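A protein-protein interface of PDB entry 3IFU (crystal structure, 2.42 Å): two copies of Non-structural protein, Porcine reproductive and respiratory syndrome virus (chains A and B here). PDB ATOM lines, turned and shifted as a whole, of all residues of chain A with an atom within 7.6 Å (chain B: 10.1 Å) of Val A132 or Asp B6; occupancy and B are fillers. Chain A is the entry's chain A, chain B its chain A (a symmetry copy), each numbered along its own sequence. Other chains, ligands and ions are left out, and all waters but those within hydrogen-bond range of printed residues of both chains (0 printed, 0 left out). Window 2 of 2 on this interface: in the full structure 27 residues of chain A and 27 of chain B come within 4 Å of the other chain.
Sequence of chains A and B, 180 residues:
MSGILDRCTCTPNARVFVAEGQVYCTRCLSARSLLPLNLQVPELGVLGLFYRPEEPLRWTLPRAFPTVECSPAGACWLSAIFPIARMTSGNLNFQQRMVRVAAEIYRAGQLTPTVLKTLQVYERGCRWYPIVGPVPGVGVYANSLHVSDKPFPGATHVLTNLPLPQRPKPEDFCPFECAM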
ATOM      1  N   TYR A 129      13.660  25.024 -19.226  1.00  0.00           N
ATOM      2  CA  TYR A 129      13.020  24.329 -18.121  1.00  0.00           C
ATOM      3  C   TYR A 129      11.583  24.039 -18.495  1.00  0.00           C
ATOM      4  O   TYR A 129      10.931  24.851 -19.163  1.00  0.00           O
ATOM      5  CB  TYR A 129      13.020  25.187 -16.857  1.00  0.00           C
ATOM      6  CG  TYR A 129      14.380  25.468 -16.264  1.00  0.00           C
ATOM      7  CD1 TYR A 129      14.917  24.641 -15.282  1.00  0.00           C
ATOM      8  CD2 TYR A 129      15.128  26.567 -16.683  1.00  0.00           C
ATOM      9  CE1 TYR A 129      16.165  24.902 -14.727  1.00  0.00           C
ATOM     10  CE2 TYR A 129      16.376  26.836 -16.140  1.00  0.00           C
ATOM     11  CZ  TYR A 129      16.893  26.004 -15.162  1.00  0.00           C
ATOM     12  OH  TYR A 129      18.134  26.271 -14.623  1.00  0.00           O
ATOM     13  N   PRO A 130      11.074  22.863 -18.098  1.00  0.00           N
ATOM     14  CA  PRO A 130       9.684  22.506 -18.403  1.00  0.00           C
ATOM     15  C   PRO A 130       8.850  23.390 -17.490  1.00  0.00           C
ATOM     16  O   PRO A 130       9.060  23.390 -16.283  1.00  0.00           O
ATOM     17  CB  PRO A 130       9.602  21.040 -17.991  1.00  0.00           C
ATOM     18  CG  PRO A 130      11.015  20.555 -18.176  1.00  0.00           C
ATOM     19  CD  PRO A 130      11.822  21.692 -17.610  1.00  0.00           C
ATOM     20  N   ILE A 131       7.926  24.157 -18.051  1.00  0.00           N
ATOM     21  CA  ILE A 131       7.113  25.032 -17.218  1.00  0.00           C
ATOM     22  C   ILE A 131       6.279  24.199 -16.249  1.00  0.00           C
ATOM     23  O   ILE A 131       5.552  23.299 -16.661  1.00  0.00           O
ATOM     24  CB  ILE A 131       6.178  25.920 -18.068  1.00  0.00           C
ATOM     25  CG1 ILE A 131       7.002  26.823 -18.988  1.00  0.00           C
ATOM     26  CG2 ILE A 131       5.306  26.761 -17.158  1.00  0.00           C
ATOM     27  CD1 ILE A 131       6.182  27.515 -20.067  1.00  0.00           C
ATOM     28  N   VAL A 132       6.405  24.497 -14.960  1.00  0.00           N
ATOM     29  CA  VAL A 132       5.672  23.789 -13.915  1.00  0.00           C
ATOM     30  C   VAL A 132       5.098  24.781 -12.919  1.00  0.00           C
ATOM     31  O   VAL A 132       4.545  24.391 -11.892  1.00  0.00           O
ATOM     32  CB  VAL A 132       6.584  22.807 -13.136  1.00  0.00           C
ATOM     33  CG1 VAL A 132       6.810  21.547 -13.943  1.00  0.00           C
ATOM     34  CG2 VAL A 132       7.911  23.483 -12.810  1.00  0.00           C
ATOM     35  N   GLY A 133       5.239  26.064 -13.232  1.00  0.00           N
ATOM     36  CA  GLY A 133       4.750  27.111 -12.357  1.00  0.00           C
ATOM     37  C   GLY A 133       5.296  28.470 -12.756  1.00  0.00           C
ATOM     38  O   GLY A 133       6.001  28.588 -13.754  1.00  0.00           O
ATOM     39  N   PRO A 134       5.002  29.518 -11.982  1.00  0.00           N
ATOM     40  CA  PRO A 134       5.472  30.873 -12.276  1.00  0.00           C
ATOM     41  C   PRO A 134       6.985  31.055 -12.154  1.00  0.00           C
ATOM     42  O   PRO A 134       7.621  30.491 -11.274  1.00  0.00           O
ATOM     43  CB  PRO A 134       4.727  31.733 -11.249  1.00  0.00           C
ATOM     44  CG  PRO A 134       3.589  30.865 -10.782  1.00  0.00           C
ATOM     45  CD  PRO A 134       4.195  29.504 -10.752  1.00  0.00           C
ATOM     46  N   VAL A 135       7.554  31.847 -13.054  1.00  0.00           N
ATOM     47  CA  VAL A 135       8.983  32.143 -13.019  1.00  0.00           C
ATOM     48  C   VAL A 135       9.144  33.655 -13.002  1.00  0.00           C
ATOM     49  O   VAL A 135       8.601  34.357 -13.853  1.00  0.00           O
ATOM     50  CB  VAL A 135       9.734  31.594 -14.242  1.00  0.00           C
ATOM     51  CG1 VAL A 135      11.207  32.047 -14.190  1.00  0.00           C
ATOM     52  CG2 VAL A 135       9.649  30.077 -14.259  1.00  0.00           C
ATOM     53  N   THR A 156       5.439  25.464 -23.214  1.00  0.00           N
ATOM     54  CA  THR A 156       5.823  24.284 -22.453  1.00  0.00           C
ATOM     55  C   THR A 156       7.196  24.434 -21.812  1.00  0.00           C
ATOM     56  O   THR A 156       7.538  23.698 -20.892  1.00  0.00           O
ATOM     57  CB  THR A 156       5.862  23.030 -23.355  1.00  0.00           C
ATOM     58  OG1 THR A 156       6.958  23.141 -24.268  1.00  0.00           O
ATOM     59  CG2 THR A 156       4.573  22.902 -24.153  1.00  0.00           C
ATOM     60  N   HIS A 157       7.982  25.386 -22.299  1.00  0.00           N
ATOM     61  CA  HIS A 157       9.318  25.595 -21.757  1.00  0.00           C
ATOM     62  C   HIS A 157       9.684  27.055 -21.557  1.00  0.00           C
ATOM     63  O   HIS A 157       9.160  27.942 -22.228  1.00  0.00           O
ATOM     64  CB  HIS A 157      10.348  24.935 -22.671  1.00  0.00           C
ATOM     65  CG  HIS A 157      10.198  23.451 -22.756  1.00  0.00           C
ATOM     66  ND1 HIS A 157      10.641  22.604 -21.764  1.00  0.00           N
ATOM     67  CD2 HIS A 157       9.577  22.670 -23.671  1.00  0.00           C
ATOM     68  CE1 HIS A 157      10.293  21.365 -22.061  1.00  0.00           C
ATOM     69  NE2 HIS A 157       9.647  21.378 -23.212  1.00  0.00           N
ATOM     70  N   VAL A 158      10.587  27.295 -20.614  1.00  0.00           N
ATOM     71  CA  VAL A 158      11.048  28.644 -20.336  1.00  0.00           C
ATOM     72  C   VAL A 158      12.567  28.649 -20.276  1.00  0.00           C
ATOM     73  O   VAL A 158      13.178  27.825 -19.601  1.00  0.00           O
ATOM     74  CB  VAL A 158      10.476  29.175 -19.010  1.00  0.00           C
ATOM     75  CG1 VAL A 158      10.901  28.279 -17.861  1.00  0.00           C
ATOM     76  CG2 VAL A 158      10.934  30.614 -18.787  1.00  0.00           C
ATOM     77  N   LEU A 164      17.014  28.052 -11.177  1.00  0.00           N
ATOM     78  CA  LEU A 164      15.753  27.411 -10.815  1.00  0.00           C
ATOM     79  C   LEU A 164      15.857  26.068 -10.086  1.00  0.00           C
ATOM     80  O   LEU A 164      16.888  25.400 -10.145  1.00  0.00           O
ATOM     81  CB  LEU A 164      14.883  27.256 -12.068  1.00  0.00           C
ATOM     82  CG  LEU A 164      14.466  28.571 -12.734  1.00  0.00           C
ATOM     83  CD1 LEU A 164      13.471  28.274 -13.853  1.00  0.00           C
ATOM     84  CD2 LEU A 164      13.850  29.508 -11.702  1.00  0.00           C
ATOM     85  N   PRO A 165      14.774  25.657  -9.393  1.00  0.00           N
ATOM     86  CA  PRO A 165      14.702  24.402  -8.637  1.00  0.00           C
ATOM     87  C   PRO A 165      14.494  23.179  -9.532  1.00  0.00           C
ATOM     88  O   PRO A 165      14.970  22.090  -9.223  1.00  0.00           O
ATOM     89  CB  PRO A 165      13.523  24.641  -7.704  1.00  0.00           C
ATOM     90  CG  PRO A 165      12.584  25.366  -8.589  1.00  0.00           C
ATOM     91  CD  PRO A 165      13.502  26.395  -9.264  1.00  0.00           C
ATOM     92  N   GLN A 166      13.773  23.359 -10.634  1.00  0.00           N
ATOM     93  CA  GLN A 166      13.535  22.262 -11.564  1.00  0.00           C
ATOM     94  C   GLN A 166      14.879  21.771 -12.076  1.00  0.00           C
ATOM     95  O   GLN A 166      15.930  22.261 -11.659  1.00  0.00           O
ATOM     96  CB  GLN A 166      12.687  22.723 -12.758  1.00  0.00           C
ATOM     97  CG  GLN A 166      11.309  23.239 -12.394  1.00  0.00           C
ATOM     98  CD  GLN A 166      11.128  24.708 -12.727  1.00  0.00           C
ATOM     99  OE1 GLN A 166      11.130  25.096 -13.897  1.00  0.00           O
ATOM    100  NE2 GLN A 166      10.975  25.536 -11.695  1.00  0.00           N
ATOM    101  N   ARG A 167      14.842  20.810 -12.992  1.00  0.00           N
ATOM    102  CA  ARG A 167      16.065  20.261 -13.555  1.00  0.00           C
ATOM    103  C   ARG A 167      16.217  20.762 -14.982  1.00  0.00           C
ATOM    104  O   ARG A 167      15.343  20.551 -15.822  1.00  0.00           O
ATOM    105  CB  ARG A 167      16.013  18.731 -13.534  1.00  0.00           C
ATOM    106  CG  ARG A 167      15.136  18.162 -12.421  1.00  0.00           C
ATOM    107  CD  ARG A 167      15.432  16.691 -12.138  1.00  0.00           C
ATOM    108  NE  ARG A 167      15.796  15.950 -13.345  1.00  0.00           N
ATOM    109  CZ  ARG A 167      17.026  15.519 -13.610  1.00  0.00           C
ATOM    110  NH1 ARG A 167      17.273  14.856 -14.733  1.00  0.00           N
ATOM    111  NH2 ARG A 167      18.005  15.742 -12.742  1.00  0.00           N
ATOM    112  N   ASP B   6       3.109  22.416  -8.610  1.00  0.00           N
ATOM    113  CA  ASP B   6       4.510  22.456  -8.097  1.00  0.00           C
ATOM    114  C   ASP B   6       4.789  23.834  -7.498  1.00  0.00           C
ATOM    115  O   ASP B   6       4.976  24.822  -8.213  1.00  0.00           O
ATOM    116  CB  ASP B   6       5.495  22.149  -9.228  1.00  0.00           C
ATOM    117  CG  ASP B   6       6.840  21.666  -8.714  1.00  0.00           C
ATOM    118  OD1 ASP B   6       6.863  20.694  -7.922  1.00  0.00           O
ATOM    119  OD2 ASP B   6       7.870  22.255  -9.105  1.00  0.00           O
ATOM    120  N   ARG B   7       4.811  23.871  -6.170  1.00  0.00           N
ATOM    121  CA  ARG B   7       5.013  25.093  -5.398  1.00  0.00           C
ATOM    122  C   ARG B   7       6.264  24.995  -4.526  1.00  0.00           C
ATOM    123  O   ARG B   7       7.027  24.039  -4.628  1.00  0.00           O
ATOM    124  CB  ARG B   7       3.791  25.314  -4.500  1.00  0.00           C
ATOM    125  CG  ARG B   7       3.119  26.672  -4.615  1.00  0.00           C
ATOM    126  CD  ARG B   7       2.386  26.882  -5.934  1.00  0.00           C
ATOM    127  NE  ARG B   7       1.598  28.113  -5.894  1.00  0.00           N
ATOM    128  CZ  ARG B   7       0.983  28.655  -6.943  1.00  0.00           C
ATOM    129  NH1 ARG B   7       1.060  28.076  -8.136  1.00  0.00           N
ATOM    130  NH2 ARG B   7       0.293  29.782  -6.799  1.00  0.00           N
ATOM    131  N   CYS B   8       6.462  25.989  -3.667  1.00  0.00           N
ATOM    132  CA  CYS B   8       7.601  26.009  -2.760  1.00  0.00           C
ATOM    133  C   CYS B   8       7.334  25.088  -1.575  1.00  0.00           C
ATOM    134  O   CYS B   8       6.231  25.083  -1.026  1.00  0.00           O
ATOM    135  CB  CYS B   8       7.850  27.427  -2.247  1.00  0.00           C
ATOM    136  SG  CYS B   8       8.747  27.486  -0.669  1.00  0.00           S
ATOM    137  N   THR B   9       8.345  24.326  -1.174  1.00  0.00           N
ATOM    138  CA  THR B   9       8.200  23.403  -0.056  1.00  0.00           C
ATOM    139  C   THR B   9       9.310  23.580   0.968  1.00  0.00           C
ATOM    140  O   THR B   9       9.824  22.601   1.504  1.00  0.00           O
ATOM    141  CB  THR B   9       8.224  21.934  -0.520  1.00  0.00           C
ATOM    142  OG1 THR B   9       7.434  21.792  -1.703  1.00  0.00           O
ATOM    143  CG2 THR B   9       7.647  21.027   0.568  1.00  0.00           C
ATOM    144  N   CYS B  10       9.687  24.826   1.223  1.00  0.00           N
ATOM    145  CA  CYS B  10      10.725  25.124   2.202  1.00  0.00           C
ATOM    146  C   CYS B  10      10.052  25.363   3.548  1.00  0.00           C
ATOM    147  O   CYS B  10       8.827  25.454   3.625  1.00  0.00           O
ATOM    148  CB  CYS B  10      11.501  26.383   1.797  1.00  0.00           C
ATOM    149  SG  CYS B  10      12.598  26.217   0.369  1.00  0.00           S
ATOM    150  N   GLN B  22       2.697  37.263  -8.334  1.00  0.00           N
ATOM    151  CA  GLN B  22       3.220  36.205  -7.471  1.00  0.00           C
ATOM    152  C   GLN B  22       4.125  36.515  -6.287  1.00  0.00           C
ATOM    153  O   GLN B  22       4.984  37.393  -6.321  1.00  0.00           O
ATOM    154  CB  GLN B  22       3.957  35.152  -8.311  1.00  0.00           C
ATOM    155  CG  GLN B  22       3.089  34.064  -8.917  1.00  0.00           C
ATOM    156  CD  GLN B  22       2.287  33.309  -7.884  1.00  0.00           C
ATOM    157  OE1 GLN B  22       2.804  32.920  -6.824  1.00  0.00           O
ATOM    158  NE2 GLN B  22       1.011  33.079  -8.188  1.00  0.00           N
ATOM    159  N   VAL B  23       3.917  35.718  -5.249  1.00  0.00           N
ATOM    160  CA  VAL B  23       4.685  35.757  -4.027  1.00  0.00           C
ATOM    161  C   VAL B  23       5.645  34.597  -4.276  1.00  0.00           C
ATOM    162  O   VAL B  23       5.212  33.488  -4.596  1.00  0.00           O
ATOM    163  CB  VAL B  23       3.774  35.449  -2.814  1.00  0.00           C
ATOM    164  CG1 VAL B  23       4.589  35.305  -1.554  1.00  0.00           C
ATOM    165  CG2 VAL B  23       2.754  36.559  -2.646  1.00  0.00           C
ATOM    166  N   TYR B  24       6.943  34.854  -4.182  1.00  0.00           N
ATOM    167  CA  TYR B  24       7.937  33.807  -4.415  1.00  0.00           C
ATOM    168  C   TYR B  24       8.806  33.609  -3.188  1.00  0.00           C
ATOM    169  O   TYR B  24       8.940  34.505  -2.362  1.00  0.00           O
ATOM    170  CB  TYR B  24       8.862  34.155  -5.593  1.00  0.00           C
ATOM    171  CG  TYR B  24       8.239  34.184  -6.977  1.00  0.00           C
ATOM    172  CD1 TYR B  24       7.704  35.358  -7.504  1.00  0.00           C
ATOM    173  CD2 TYR B  24       8.232  33.042  -7.779  1.00  0.00           C
ATOM    174  CE1 TYR B  24       7.185  35.395  -8.799  1.00  0.00           C
ATOM    175  CE2 TYR B  24       7.715  33.066  -9.072  1.00  0.00           C
ATOM    176  CZ  TYR B  24       7.196  34.241  -9.576  1.00  0.00           C
ATOM    177  OH  TYR B  24       6.707  34.257 -10.861  1.00  0.00           O
ATOM    178  N   CYS B  28      14.194  29.042  -2.840  1.00  0.00           N
ATOM    179  CA  CYS B  28      14.126  28.205  -4.040  1.00  0.00           C
ATOM    180  C   CYS B  28      13.548  28.880  -5.279  1.00  0.00           C
ATOM    181  O   CYS B  28      13.465  28.255  -6.336  1.00  0.00           O
ATOM    182  CB  CYS B  28      13.312  26.943  -3.752  1.00  0.00           C
ATOM    183  SG  CYS B  28      11.557  27.253  -3.463  1.00  0.00           S
ATOM    184  N   LEU B  29      13.130  30.138  -5.145  1.00  0.00           N
ATOM    185  CA  LEU B  29      12.579  30.896  -6.267  1.00  0.00           C
ATOM    186  C   LEU B  29      11.300  30.294  -6.854  1.00  0.00           C
ATOM    187  O   LEU B  29      10.938  30.578  -7.996  1.00  0.00           O
ATOM    188  CB  LEU B  29      13.640  31.033  -7.361  1.00  0.00           C
ATOM    189  CG  LEU B  29      14.989  31.545  -6.850  1.00  0.00           C
ATOM    190  CD1 LEU B  29      16.080  31.368  -7.901  1.00  0.00           C
ATOM    191  CD2 LEU B  29      14.835  33.000  -6.451  1.00  0.00           C
ATOM    192  N   SER B  30      10.616  29.462  -6.074  1.00  0.00           N
ATOM    193  CA  SER B  30       9.375  28.850  -6.529  1.00  0.00           C
ATOM    194  C   SER B  30       8.208  29.597  -5.913  1.00  0.00           C
ATOM    195  O   SER B  30       8.335  30.151  -4.819  1.00  0.00           O
ATOM    196  CB  SER B  30       9.323  27.382  -6.115  1.00  0.00           C
ATOM    197  OG  SER B  30      10.425  26.667  -6.649  1.00  0.00           O
ATOM    198  N   ALA B  31       7.076  29.616  -6.613  1.00  0.00           N
ATOM    199  CA  ALA B  31       5.876  30.296  -6.124  1.00  0.00           C
ATOM    200  C   ALA B  31       5.503  29.824  -4.721  1.00  0.00           C
ATOM    201  O   ALA B  31       5.608  28.641  -4.409  1.00  0.00           O
ATOM    202  CB  ALA B  31       4.715  30.054  -7.079  1.00  0.00           C
ATOM    203  N   ARG B  32       5.065  30.752  -3.881  1.00  0.00           N
ATOM    204  CA  ARG B  32       4.680  30.425  -2.513  1.00  0.00           C
ATOM    205  C   ARG B  32       3.176  30.406  -2.289  1.00  0.00           C
ATOM    206  O   ARG B  32       2.481  31.379  -2.578  1.00  0.00           O
ATOM    207  CB  ARG B  32       5.316  31.417  -1.541  1.00  0.00           C
ATOM    208  CG  ARG B  32       6.479  30.841  -0.775  1.00  0.00           C
ATOM    209  CD  ARG B  32       6.004  30.058   0.427  1.00  0.00           C
ATOM    210  NE  ARG B  32       6.402  30.722   1.666  1.00  0.00           N
ATOM    211  CZ  ARG B  32       7.663  30.885   2.057  1.00  0.00           C
ATOM    212  NH1 ARG B  32       8.661  30.432   1.311  1.00  0.00           N
ATOM    213  NH2 ARG B  32       7.929  31.502   3.194  1.00  0.00           N
ATOM    214  N   SER B  33       2.682  29.293  -1.762  1.00  0.00           N
ATOM    215  CA  SER B  33       1.262  29.150  -1.477  1.00  0.00           C
ATOM    216  C   SER B  33       0.895  29.868  -0.186  1.00  0.00           C
ATOM    217  O   SER B  33       1.759  30.358   0.539  1.00  0.00           O
ATOM    218  CB  SER B  33       0.880  27.671  -1.357  1.00  0.00           C
ATOM    219  OG  SER B  33       0.826  27.044  -2.627  1.00  0.00           O
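OH of Tyr B24 sits close to N of Val A135.
O of Ala B31 sits at hydrogen-bond distance from N of Cys B8, at 2.9 Å.
O of Cys B28 lies within hydrogen-bond range of OG of Ser B30.
Among the printed residues, merely in contact across the chains: Pro A165 with Ser B30 (3.2 Å), Pro A134 with Tyr B24 (3.2 Å), Pro A165 with Cys B28 (3.5 Å), Val A132 with Asp B6 (3.6 Å), Pro A134 with Gln B22 (3.7 Å) and Pro A134 with Ala B31 (3.8 Å).
No residue of chain B comes within 4 Å of Ile A131.
Of chain B, only Asp B6 (3.6 Å) comes within 4 Å of Val A132.
Printed residues of chain B within 4 Å of Val A135: Tyr B24 (3.3 Å).
Asp B6 touches just one residue of chain A: Val A132 (3.6 Å).
Of the printed residues of chain A, Ala B31 touches Pro A134.
The nearest residue of chain B that does not touch Val A132 is Arg B7 (5.8 Å).
The nearest printed residue of chain B that does not touch Val A135 is Leu B29 (5.6 Å).
Of the 14 printed residues of chain A, 4 touch a printed residue of chain B.
Along chain A the printed residues that touch a printed residue of chain B span positions 132 to 165.
Hydrophobic or aromatic side chains of chain B that line the printed part of chain A: Tyr B24 and Ala B31.
Among the printed residues, 7 pairs touch across the chains.
Among the printed residues, no Asp or Glu carboxylate lies within 4 Å of a Lys or Arg side-chain nitrogen of the other chain.
No position is printed for both chains.
Of the 7 pairs that touch across the chains among the printed residues, none has its exchanged pair printed and touching as well.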
